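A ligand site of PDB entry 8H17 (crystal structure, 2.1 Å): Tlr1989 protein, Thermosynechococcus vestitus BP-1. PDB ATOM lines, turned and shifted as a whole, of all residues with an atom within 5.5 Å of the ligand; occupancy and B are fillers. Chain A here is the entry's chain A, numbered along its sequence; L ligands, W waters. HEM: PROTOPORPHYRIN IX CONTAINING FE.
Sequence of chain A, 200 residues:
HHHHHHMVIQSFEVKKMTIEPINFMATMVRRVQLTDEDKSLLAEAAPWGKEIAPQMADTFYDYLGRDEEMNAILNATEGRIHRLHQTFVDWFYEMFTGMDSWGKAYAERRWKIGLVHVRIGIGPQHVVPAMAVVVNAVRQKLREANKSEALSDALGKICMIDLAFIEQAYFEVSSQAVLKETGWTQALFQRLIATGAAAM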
ATOM      1  N   PHE A  60      29.222  29.342 -23.383  1.00  0.00           N
ATOM      2  CA  PHE A  60      28.416  28.486 -24.272  1.00  0.00           C
ATOM      3  C   PHE A  60      28.590  28.959 -25.715  1.00  0.00           C
ATOM      4  O   PHE A  60      28.884  28.146 -26.625  1.00  0.00           O
ATOM      5  CB  PHE A  60      26.945  28.508 -23.861  1.00  0.00           C
ATOM      6  CG  PHE A  60      26.140  27.377 -24.444  1.00  0.00           C
ATOM      7  CD1 PHE A  60      26.587  26.064 -24.359  1.00  0.00           C
ATOM      8  CD2 PHE A  60      24.998  27.654 -25.173  1.00  0.00           C
ATOM      9  CE1 PHE A  60      25.843  25.027 -24.911  1.00  0.00           C
ATOM     10  CE2 PHE A  60      24.250  26.627 -25.726  1.00  0.00           C
ATOM     11  CZ  PHE A  60      24.653  25.314 -25.578  1.00  0.00           C
ATOM     12  N   LEU A  64      30.101  26.833 -28.818  1.00  0.00           N
ATOM     13  CA  LEU A  64      29.379  26.559 -30.100  1.00  0.00           C
ATOM     14  C   LEU A  64      30.257  27.071 -31.261  1.00  0.00           C
ATOM     15  O   LEU A  64      30.363  26.380 -32.297  1.00  0.00           O
ATOM     16  CB  LEU A  64      28.017  27.262 -30.108  1.00  0.00           C
ATOM     17  CG  LEU A  64      27.013  26.776 -29.061  1.00  0.00           C
ATOM     18  CD1 LEU A  64      25.719  27.579 -29.148  1.00  0.00           C
ATOM     19  CD2 LEU A  64      26.707  25.273 -29.195  1.00  0.00           C
ATOM     20  N   MET A  70      28.344  23.418 -35.794  1.00  0.00           N
ATOM     21  CA  MET A  70      27.398  24.240 -34.963  1.00  0.00           C
ATOM     22  C   MET A  70      27.610  25.740 -35.243  1.00  0.00           C
ATOM     23  O   MET A  70      26.644  26.499 -35.178  1.00  0.00           O
ATOM     24  CB  MET A  70      27.536  23.932 -33.473  1.00  0.00           C
ATOM     25  CG  MET A  70      27.323  22.442 -33.204  1.00  0.00           C
ATOM     26  SD  MET A  70      27.132  22.024 -31.469  1.00  0.00           S
ATOM     27  CE  MET A  70      28.811  22.162 -30.856  1.00  0.00           C
ATOM     28  N   ILE A  73      25.618  26.544 -38.285  1.00  0.00           N
ATOM     29  CA  ILE A  73      24.176  26.697 -37.921  1.00  0.00           C
ATOM     30  C   ILE A  73      23.952  28.091 -37.324  1.00  0.00           C
ATOM     31  O   ILE A  73      22.887  28.674 -37.572  1.00  0.00           O
ATOM     32  CB  ILE A  73      23.723  25.526 -37.025  1.00  0.00           C
ATOM     33  CG1 ILE A  73      23.636  24.211 -37.811  1.00  0.00           C
ATOM     34  CG2 ILE A  73      22.409  25.855 -36.332  1.00  0.00           C
ATOM     35  CD1 ILE A  73      24.007  22.968 -37.029  1.00  0.00           C
ATOM     36  N   LEU A  74      24.921  28.651 -36.618  1.00  0.00           N
ATOM     37  CA  LEU A  74      24.678  29.969 -35.964  1.00  0.00           C
ATOM     38  C   LEU A  74      25.050  31.100 -36.925  1.00  0.00           C
ATOM     39  O   LEU A  74      25.836  31.962 -36.518  1.00  0.00           O
ATOM     40  CB  LEU A  74      25.544  30.046 -34.707  1.00  0.00           C
ATOM     41  CG  LEU A  74      25.131  29.156 -33.541  1.00  0.00           C
ATOM     42  CD1 LEU A  74      25.947  29.499 -32.313  1.00  0.00           C
ATOM     43  CD2 LEU A  74      23.649  29.313 -33.254  1.00  0.00           C
ATOM     44  N   ARG A  80      21.909  38.074 -34.244  1.00  0.00           N
ATOM     45  CA  ARG A  80      21.686  36.761 -33.591  1.00  0.00           C
ATOM     46  C   ARG A  80      22.539  36.677 -32.325  1.00  0.00           C
ATOM     47  O   ARG A  80      22.083  36.056 -31.351  1.00  0.00           O
ATOM     48  CB  ARG A  80      22.038  35.647 -34.571  1.00  0.00           C
ATOM     49  CG  ARG A  80      21.234  34.365 -34.360  1.00  0.00           C
ATOM     50  CD  ARG A  80      21.611  33.289 -35.366  1.00  0.00           C
ATOM     51  NE  ARG A  80      20.453  32.548 -35.822  1.00  0.00           N
ATOM     52  CZ  ARG A  80      20.505  31.535 -36.685  1.00  0.00           C
ATOM     53  NH1 ARG A  80      19.385  30.917 -37.042  1.00  0.00           N
ATOM     54  NH2 ARG A  80      21.662  31.147 -37.173  1.00  0.00           N
ATOM     55  N   ARG A  83      20.746  37.911 -29.293  1.00  0.00           N
ATOM     56  CA  ARG A  83      19.554  37.066 -29.032  1.00  0.00           C
ATOM     57  C   ARG A  83      20.018  35.714 -28.446  1.00  0.00           C
ATOM     58  O   ARG A  83      19.405  35.252 -27.480  1.00  0.00           O
ATOM     59  CB  ARG A  83      18.736  36.991 -30.321  1.00  0.00           C
ATOM     60  CG  ARG A  83      17.927  35.706 -30.488  1.00  0.00           C
ATOM     61  CD  ARG A  83      16.556  35.906 -31.117  1.00  0.00           C
ATOM     62  NE  ARG A  83      15.550  36.309 -30.133  1.00  0.00           N
ATOM     63  CZ  ARG A  83      14.682  35.505 -29.498  1.00  0.00           C
ATOM     64  NH1 ARG A  83      13.831  36.023 -28.639  1.00  0.00           N
ATOM     65  NH2 ARG A  83      14.668  34.196 -29.701  1.00  0.00           N
ATOM     66  N   LEU A  84      21.092  35.127 -28.999  1.00  0.00           N
ATOM     67  CA  LEU A  84      21.705  33.856 -28.558  1.00  0.00           C
ATOM     68  C   LEU A  84      22.232  34.025 -27.130  1.00  0.00           C
ATOM     69  O   LEU A  84      22.137  33.034 -26.352  1.00  0.00           O
ATOM     70  CB  LEU A  84      22.852  33.449 -29.485  1.00  0.00           C
ATOM     71  CG  LEU A  84      22.459  33.029 -30.899  1.00  0.00           C
ATOM     72  CD1 LEU A  84      23.680  32.548 -31.690  1.00  0.00           C
ATOM     73  CD2 LEU A  84      21.364  31.968 -30.895  1.00  0.00           C
ATOM     74  N   THR A  87      18.722  34.798 -24.808  1.00  0.00           N
ATOM     75  CA  THR A  87      17.837  33.621 -24.694  1.00  0.00           C
ATOM     76  C   THR A  87      18.453  32.670 -23.673  1.00  0.00           C
ATOM     77  O   THR A  87      17.726  32.232 -22.769  1.00  0.00           O
ATOM     78  CB  THR A  87      17.543  32.995 -26.048  1.00  0.00           C
ATOM     79  OG1 THR A  87      18.791  32.681 -26.641  1.00  0.00           O
ATOM     80  CG2 THR A  87      16.697  33.926 -26.887  1.00  0.00           C
ATOM     81  N   PHE A  88      19.778  32.508 -23.734  1.00  0.00           N
ATOM     82  CA  PHE A  88      20.550  31.586 -22.858  1.00  0.00           C
ATOM     83  C   PHE A  88      20.483  32.093 -21.418  1.00  0.00           C
ATOM     84  O   PHE A  88      20.220  31.277 -20.509  1.00  0.00           O
ATOM     85  CB  PHE A  88      21.993  31.426 -23.335  1.00  0.00           C
ATOM     86  CG  PHE A  88      22.705  30.388 -22.510  1.00  0.00           C
ATOM     87  CD1 PHE A  88      23.216  30.709 -21.268  1.00  0.00           C
ATOM     88  CD2 PHE A  88      22.839  29.090 -22.960  1.00  0.00           C
ATOM     89  CE1 PHE A  88      23.822  29.751 -20.473  1.00  0.00           C
ATOM     90  CE2 PHE A  88      23.457  28.136 -22.174  1.00  0.00           C
ATOM     91  CZ  PHE A  88      23.944  28.460 -20.926  1.00  0.00           C
ATOM     92  N   TRP A  91      16.940  31.519 -20.004  1.00  0.00           N
ATOM     93  CA  TRP A  91      16.686  30.061 -19.855  1.00  0.00           C
ATOM     94  C   TRP A  91      17.396  29.595 -18.584  1.00  0.00           C
ATOM     95  O   TRP A  91      16.773  28.944 -17.752  1.00  0.00           O
ATOM     96  CB  TRP A  91      17.160  29.265 -21.077  1.00  0.00           C
ATOM     97  CG  TRP A  91      17.369  27.827 -20.751  1.00  0.00           C
ATOM     98  CD1 TRP A  91      16.417  26.860 -20.650  1.00  0.00           C
ATOM     99  CD2 TRP A  91      18.616  27.214 -20.398  1.00  0.00           C
ATOM    100  NE1 TRP A  91      16.987  25.675 -20.298  1.00  0.00           N
ATOM    101  CE2 TRP A  91      18.327  25.857 -20.123  1.00  0.00           C
ATOM    102  CE3 TRP A  91      19.947  27.650 -20.338  1.00  0.00           C
ATOM    103  CZ2 TRP A  91      19.319  24.965 -19.746  1.00  0.00           C
ATOM    104  CZ3 TRP A  91      20.930  26.754 -19.962  1.00  0.00           C
ATOM    105  CH2 TRP A  91      20.616  25.445 -19.640  1.00  0.00           C
ATOM    106  N   ARG A 109       7.329  26.562 -21.762  1.00  0.00           N
ATOM    107  CA  ARG A 109       8.533  27.271 -22.254  1.00  0.00           C
ATOM    108  C   ARG A 109       9.584  26.242 -22.709  1.00  0.00           C
ATOM    109  O   ARG A 109      10.207  26.393 -23.815  1.00  0.00           O
ATOM    110  CB  ARG A 109       9.080  28.123 -21.108  1.00  0.00           C
ATOM    111  CG  ARG A 109      10.312  28.942 -21.483  1.00  0.00           C
ATOM    112  CD  ARG A 109      10.113  29.725 -22.792  1.00  0.00           C
ATOM    113  NE  ARG A 109      11.367  30.303 -23.264  1.00  0.00           N
ATOM    114  CZ  ARG A 109      11.605  30.670 -24.522  1.00  0.00           C
ATOM    115  NH1 ARG A 109      12.781  31.180 -24.856  1.00  0.00           N
ATOM    116  NH2 ARG A 109      10.679  30.531 -25.455  1.00  0.00           N
ATOM    117  N   LYS A 112       8.550  24.686 -25.997  1.00  0.00           N
ATOM    118  CA  LYS A 112       8.834  25.644 -27.106  1.00  0.00           C
ATOM    119  C   LYS A 112      10.346  25.664 -27.407  1.00  0.00           C
ATOM    120  O   LYS A 112      10.703  25.663 -28.592  1.00  0.00           O
ATOM    121  CB  LYS A 112       8.374  27.072 -26.797  1.00  0.00           C
ATOM    122  CG  LYS A 112       8.623  28.081 -27.923  1.00  0.00           C
ATOM    123  CD  LYS A 112       8.045  27.669 -29.279  1.00  0.00           C
ATOM    124  CE  LYS A 112       8.047  28.772 -30.328  1.00  0.00           C
ATOM    125  NZ  LYS A 112       7.303  29.953 -29.837  1.00  0.00           N
ATOM    126  N   ILE A 113      11.183  25.665 -26.379  1.00  0.00           N
ATOM    127  CA  ILE A 113      12.663  25.606 -26.595  1.00  0.00           C
ATOM    128  C   ILE A 113      13.029  24.368 -27.430  1.00  0.00           C
ATOM    129  O   ILE A 113      13.853  24.464 -28.427  1.00  0.00           O
ATOM    130  CB  ILE A 113      13.424  25.728 -25.255  1.00  0.00           C
ATOM    131  CG1 ILE A 113      13.209  27.134 -24.677  1.00  0.00           C
ATOM    132  CG2 ILE A 113      14.912  25.412 -25.408  1.00  0.00           C
ATOM    133  CD1 ILE A 113      13.692  27.279 -23.257  1.00  0.00           C
ATOM    134  N   VAL A 116      12.020  24.814 -31.114  1.00  0.00           N
ATOM    135  CA  VAL A 116      12.892  25.760 -31.850  1.00  0.00           C
ATOM    136  C   VAL A 116      14.109  24.998 -32.408  1.00  0.00           C
ATOM    137  O   VAL A 116      14.506  25.190 -33.575  1.00  0.00           O
ATOM    138  CB  VAL A 116      13.250  26.968 -30.953  1.00  0.00           C
ATOM    139  CG1 VAL A 116      14.471  27.711 -31.483  1.00  0.00           C
ATOM    140  CG2 VAL A 116      12.072  27.916 -30.826  1.00  0.00           C
ATOM    141  N   HIS A 117      14.733  24.141 -31.600  1.00  0.00           N
ATOM    142  CA  HIS A 117      15.978  23.461 -31.989  1.00  0.00           C
ATOM    143  C   HIS A 117      15.689  22.442 -33.077  1.00  0.00           C
ATOM    144  O   HIS A 117      16.533  22.348 -34.020  1.00  0.00           O
ATOM    145  CB  HIS A 117      16.650  22.898 -30.746  1.00  0.00           C
ATOM    146  CG  HIS A 117      17.149  24.019 -29.935  1.00  0.00           C
ATOM    147  ND1 HIS A 117      16.388  24.584 -28.947  1.00  0.00           N
ATOM    148  CD2 HIS A 117      18.288  24.741 -30.042  1.00  0.00           C
ATOM    149  CE1 HIS A 117      17.100  25.567 -28.412  1.00  0.00           C
ATOM    150  NE2 HIS A 117      18.250  25.691 -29.085  1.00  0.00           N
ATOM    151  N   ILE A 120      15.330  24.213 -36.503  1.00  0.00           N
ATOM    152  CA  ILE A 120      16.575  24.715 -37.139  1.00  0.00           C
ATOM    153  C   ILE A 120      17.438  23.505 -37.527  1.00  0.00           C
ATOM    154  O   ILE A 120      18.408  23.742 -38.172  1.00  0.00           O
ATOM    155  CB  ILE A 120      17.336  25.764 -36.289  1.00  0.00           C
ATOM    156  CG1 ILE A 120      18.151  25.102 -35.182  1.00  0.00           C
ATOM    157  CG2 ILE A 120      16.394  26.833 -35.743  1.00  0.00           C
ATOM    158  CD1 ILE A 120      18.450  26.013 -34.011  1.00  0.00           C
ATOM    159  N   ILE A 122      18.860  21.160 -35.613  1.00  0.00           N
ATOM    160  CA  ILE A 122      19.839  20.626 -34.638  1.00  0.00           C
ATOM    161  C   ILE A 122      19.231  19.440 -33.863  1.00  0.00           C
ATOM    162  O   ILE A 122      18.027  19.516 -33.434  1.00  0.00           O
ATOM    163  CB  ILE A 122      20.466  21.717 -33.773  1.00  0.00           C
ATOM    164  CG1 ILE A 122      19.728  21.899 -32.465  1.00  0.00           C
ATOM    165  CG2 ILE A 122      20.621  23.047 -34.490  1.00  0.00           C
ATOM    166  CD1 ILE A 122      20.643  22.450 -31.444  1.00  0.00           C
ATOM    167  N   HIS A 126      24.192  17.348 -31.197  1.00  0.00           N
ATOM    168  CA  HIS A 126      24.517  18.755 -30.825  1.00  0.00           C
ATOM    169  C   HIS A 126      24.067  19.067 -29.393  1.00  0.00           C
ATOM    170  O   HIS A 126      24.849  19.613 -28.630  1.00  0.00           O
ATOM    171  CB  HIS A 126      23.887  19.745 -31.838  1.00  0.00           C
ATOM    172  CG  HIS A 126      24.154  19.406 -33.272  1.00  0.00           C
ATOM    173  ND1 HIS A 126      23.141  19.002 -34.129  1.00  0.00           N
ATOM    174  CD2 HIS A 126      25.291  19.407 -33.999  1.00  0.00           C
ATOM    175  CE1 HIS A 126      23.640  18.763 -35.318  1.00  0.00           C
ATOM    176  NE2 HIS A 126      24.971  19.009 -35.267  1.00  0.00           N
ATOM    177  N   VAL A 127      22.817  18.776 -29.043  1.00  0.00           N
ATOM    178  CA  VAL A 127      22.203  19.247 -27.764  1.00  0.00           C
ATOM    179  C   VAL A 127      22.725  18.401 -26.589  1.00  0.00           C
ATOM    180  O   VAL A 127      22.955  18.940 -25.490  1.00  0.00           O
ATOM    181  CB  VAL A 127      20.670  19.196 -27.873  1.00  0.00           C
ATOM    182  CG1 VAL A 127      20.060  19.494 -26.532  1.00  0.00           C
ATOM    183  CG2 VAL A 127      20.193  20.200 -28.929  1.00  0.00           C
ATOM    184  N   ALA A 130      26.203  19.609 -25.870  1.00  0.00           N
ATOM    185  CA  ALA A 130      26.067  21.021 -25.440  1.00  0.00           C
ATOM    186  C   ALA A 130      25.650  20.988 -23.982  1.00  0.00           C
ATOM    187  O   ALA A 130      26.177  21.767 -23.236  1.00  0.00           O
ATOM    188  CB  ALA A 130      25.069  21.812 -26.246  1.00  0.00           C
ATOM    189  N   MET A 131      24.639  20.173 -23.647  1.00  0.00           N
ATOM    190  CA  MET A 131      24.144  20.185 -22.254  1.00  0.00           C
ATOM    191  C   MET A 131      25.245  19.655 -21.308  1.00  0.00           C
ATOM    192  O   MET A 131      25.399  20.223 -20.193  1.00  0.00           O
ATOM    193  CB  MET A 131      22.828  19.398 -22.118  1.00  0.00           C
ATOM    194  CG  MET A 131      22.194  19.604 -20.771  1.00  0.00           C
ATOM    195  SD  MET A 131      21.714  21.316 -20.344  1.00  0.00           S
ATOM    196  CE  MET A 131      20.163  21.455 -21.220  1.00  0.00           C
ATOM    197  N   VAL A 134      27.382  22.679 -20.545  1.00  0.00           N
ATOM    198  CA  VAL A 134      26.672  23.613 -19.620  1.00  0.00           C
ATOM    199  C   VAL A 134      26.847  23.081 -18.224  1.00  0.00           C
ATOM    200  O   VAL A 134      27.242  23.867 -17.360  1.00  0.00           O
ATOM    201  CB  VAL A 134      25.171  23.761 -19.917  1.00  0.00           C
ATOM    202  CG1 VAL A 134      24.456  24.515 -18.820  1.00  0.00           C
ATOM    203  CG2 VAL A 134      24.957  24.443 -21.249  1.00  0.00           C
ATOM    204  N   ILE A 166      13.879  18.817 -24.648  1.00  0.00           N
ATOM    205  CA  ILE A 166      14.417  19.115 -26.014  1.00  0.00           C
ATOM    206  C   ILE A 166      14.448  17.814 -26.829  1.00  0.00           C
ATOM    207  O   ILE A 166      14.100  17.852 -28.032  1.00  0.00           O
ATOM    208  CB  ILE A 166      15.803  19.771 -25.892  1.00  0.00           C
ATOM    209  CG1 ILE A 166      15.684  21.158 -25.277  1.00  0.00           C
ATOM    210  CG2 ILE A 166      16.533  19.785 -27.222  1.00  0.00           C
ATOM    211  CD1 ILE A 166      16.978  21.727 -24.725  1.00  0.00           C
HETATM  212  CHA HEM L   1      17.431  29.393 -29.599  1.00  0.00           C
HETATM  213  CHB HEM L   1      18.585  27.409 -25.356  1.00  0.00           C
HETATM  214  CHC HEM L   1      21.633  24.484 -27.667  1.00  0.00           C
HETATM  215  CHD HEM L   1      21.265  27.333 -31.625  1.00  0.00           C
HETATM  216  C1A HEM L   1      17.453  28.985 -28.293  1.00  0.00           C
HETATM  217  C2A HEM L   1      16.595  29.560 -27.323  1.00  0.00           C
HETATM  218  C3A HEM L   1      16.907  29.048 -26.126  1.00  0.00           C
HETATM  219  C4A HEM L   1      18.018  28.189 -26.337  1.00  0.00           C
HETATM  220  CMA HEM L   1      16.239  29.359 -24.786  1.00  0.00           C
HETATM  221  CAA HEM L   1      15.516  30.576 -27.626  1.00  0.00           C
HETATM  222  CBA HEM L   1      14.335  29.772 -28.136  1.00  0.00           C
HETATM  223  CGA HEM L   1      13.124  30.689 -28.351  1.00  0.00           C
HETATM  224  O1A HEM L   1      13.071  31.476 -29.298  1.00  0.00           O
HETATM  225  O2A HEM L   1      12.151  30.604 -27.615  1.00  0.00           O
HETATM  226  C1B HEM L   1      19.489  26.394 -25.676  1.00  0.00           C
HETATM  227  C2B HEM L   1      19.905  25.429 -24.703  1.00  0.00           C
HETATM  228  C3B HEM L   1      20.786  24.597 -25.342  1.00  0.00           C
HETATM  229  C4B HEM L   1      20.846  25.090 -26.725  1.00  0.00           C
HETATM  230  CMB HEM L   1      19.464  25.367 -23.238  1.00  0.00           C
HETATM  231  CAB HEM L   1      21.573  23.413 -24.900  1.00  0.00           C
HETATM  232  CBB HEM L   1      21.649  22.986 -23.675  1.00  0.00           C
HETATM  233  C1C HEM L   1      21.849  25.032 -28.950  1.00  0.00           C
HETATM  234  C2C HEM L   1      22.745  24.554 -29.892  1.00  0.00           C
HETATM  235  C3C HEM L   1      22.663  25.355 -30.997  1.00  0.00           C
HETATM  236  C4C HEM L   1      21.679  26.339 -30.764  1.00  0.00           C
HETATM  237  CMC HEM L   1      23.638  23.334 -29.726  1.00  0.00           C
HETATM  238  CAC HEM L   1      23.561  25.108 -32.133  1.00  0.00           C
HETATM  239  CBC HEM L   1      23.865  26.025 -32.984  1.00  0.00           C
HETATM  240  C1D HEM L   1      20.165  28.125 -31.351  1.00  0.00           C
HETATM  241  C2D HEM L   1      19.602  29.028 -32.402  1.00  0.00           C
HETATM  242  C3D HEM L   1      18.507  29.599 -31.822  1.00  0.00           C
HETATM  243  C4D HEM L   1      18.434  29.028 -30.461  1.00  0.00           C
HETATM  244  CMD HEM L   1      20.192  29.269 -33.779  1.00  0.00           C
HETATM  245  CAD HEM L   1      17.547  30.592 -32.438  1.00  0.00           C
HETATM  246  CBD HEM L   1      18.090  31.978 -32.168  1.00  0.00           C
HETATM  247  CGD HEM L   1      17.329  33.023 -32.971  1.00  0.00           C
HETATM  248  O1D HEM L   1      16.124  33.149 -32.746  1.00  0.00           O
HETATM  249  O2D HEM L   1      17.906  33.741 -33.853  1.00  0.00           O
HETATM  250  NA  HEM L   1      18.318  28.151 -27.675  1.00  0.00           N
HETATM  251  NB  HEM L   1      20.064  26.116 -26.861  1.00  0.00           N
HETATM  252  NC  HEM L   1      21.219  26.081 -29.485  1.00  0.00           N
HETATM  253  ND  HEM L   1      19.419  28.136 -30.217  1.00  0.00           N
HETATM  254 FE   HEM L   1      19.700  27.134 -28.618  1.00  0.00          FE
HETATM  255  O   HOH W   1      15.150  32.245 -23.304  1.00  0.00           O
HETATM  256  O   HOH W   2      18.012  36.520 -34.327  1.00  0.00           O
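The guanidinium group (NH2) of Arg 83 lies within salt-bridge range of an oxygen (O1A) of the ligand, 3.2 Å away.
A ring nitrogen (NE2) of His 117 is bound to an iron atom (FE) of the ligand, 2.1 Å away.
An oxygen (O2A) of the ligand is in salt-bridge range of the guanidinium group (NH2) of Arg 109 (2.6 Å).
NE of Arg 80 lies within salt-bridge range of O2D of the ligand (3.4 Å).
OG1 of Thr 87 sits at hydrogen-bond distance from O of Arg 83 (2.8 Å).
The backbone carbonyl oxygen (O) of His 117 lies within hydrogen-bond range of the backbone NH (N) of Ile 122.
A ring nitrogen (ND1) of His 117 is in hydrogen-bond range of the backbone carbonyl oxygen (O) of Ile 113, 2.6 Å away.
O of Ile 73 is in hydrogen-bond range of NH2 of Arg 80, at 2.8 Å.
The backbone carbonyl oxygen of Leu 84 sits at hydrogen-bond distance from the side-chain hydroxyl of Thr 87, 3.4 Å away.
CZ of Phe 60 touches CAB of the ligand, at 3.7 Å.
CD2 of Leu 64 touches CMC of the ligand, 3.7 Å away.
Met 70 touches the ligand.
CG2 of Ile 73 touches CBC of the ligand, at 3.7 Å.
Leu 74 touches the ligand (CD2 to CBC, 3.3 Å).
Leu 84 touches the ligand (CD2 to CBD, 3.5 Å).
Thr 87 touches the ligand.
CE2 of Trp 91 touches CMB of the ligand (3.4 Å).
Ile 113 touches the ligand.
Val 116 touches the ligand.
CD1 of Ile 120 touches C2D of the ligand, 3.6 Å away.
Ile 122 touches the ligand (CD1 to C2C, 3.4 Å).
Met 131 touches the ligand.
Hydrophobic or aromatic side chains within 4 Å of the ligand: Phe 60, Leu 64, Ile 73, Leu 74, Leu 84, Trp 91, Ile 113, Val 116, His 117, Ile 120, Ile 122 and Met 131.
Of the 24 residues printed, 17 come within 4 Å of the ligand.
The nearest printed residue that does not touch the ligand is Ala 130 (4.1 Å).
Water W1 lies within hydrogen-bond range of the backbone carbonyl oxygen of Thr 87 (2.6 Å) and the guanidinium group of Arg 109 (3.0 Å).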
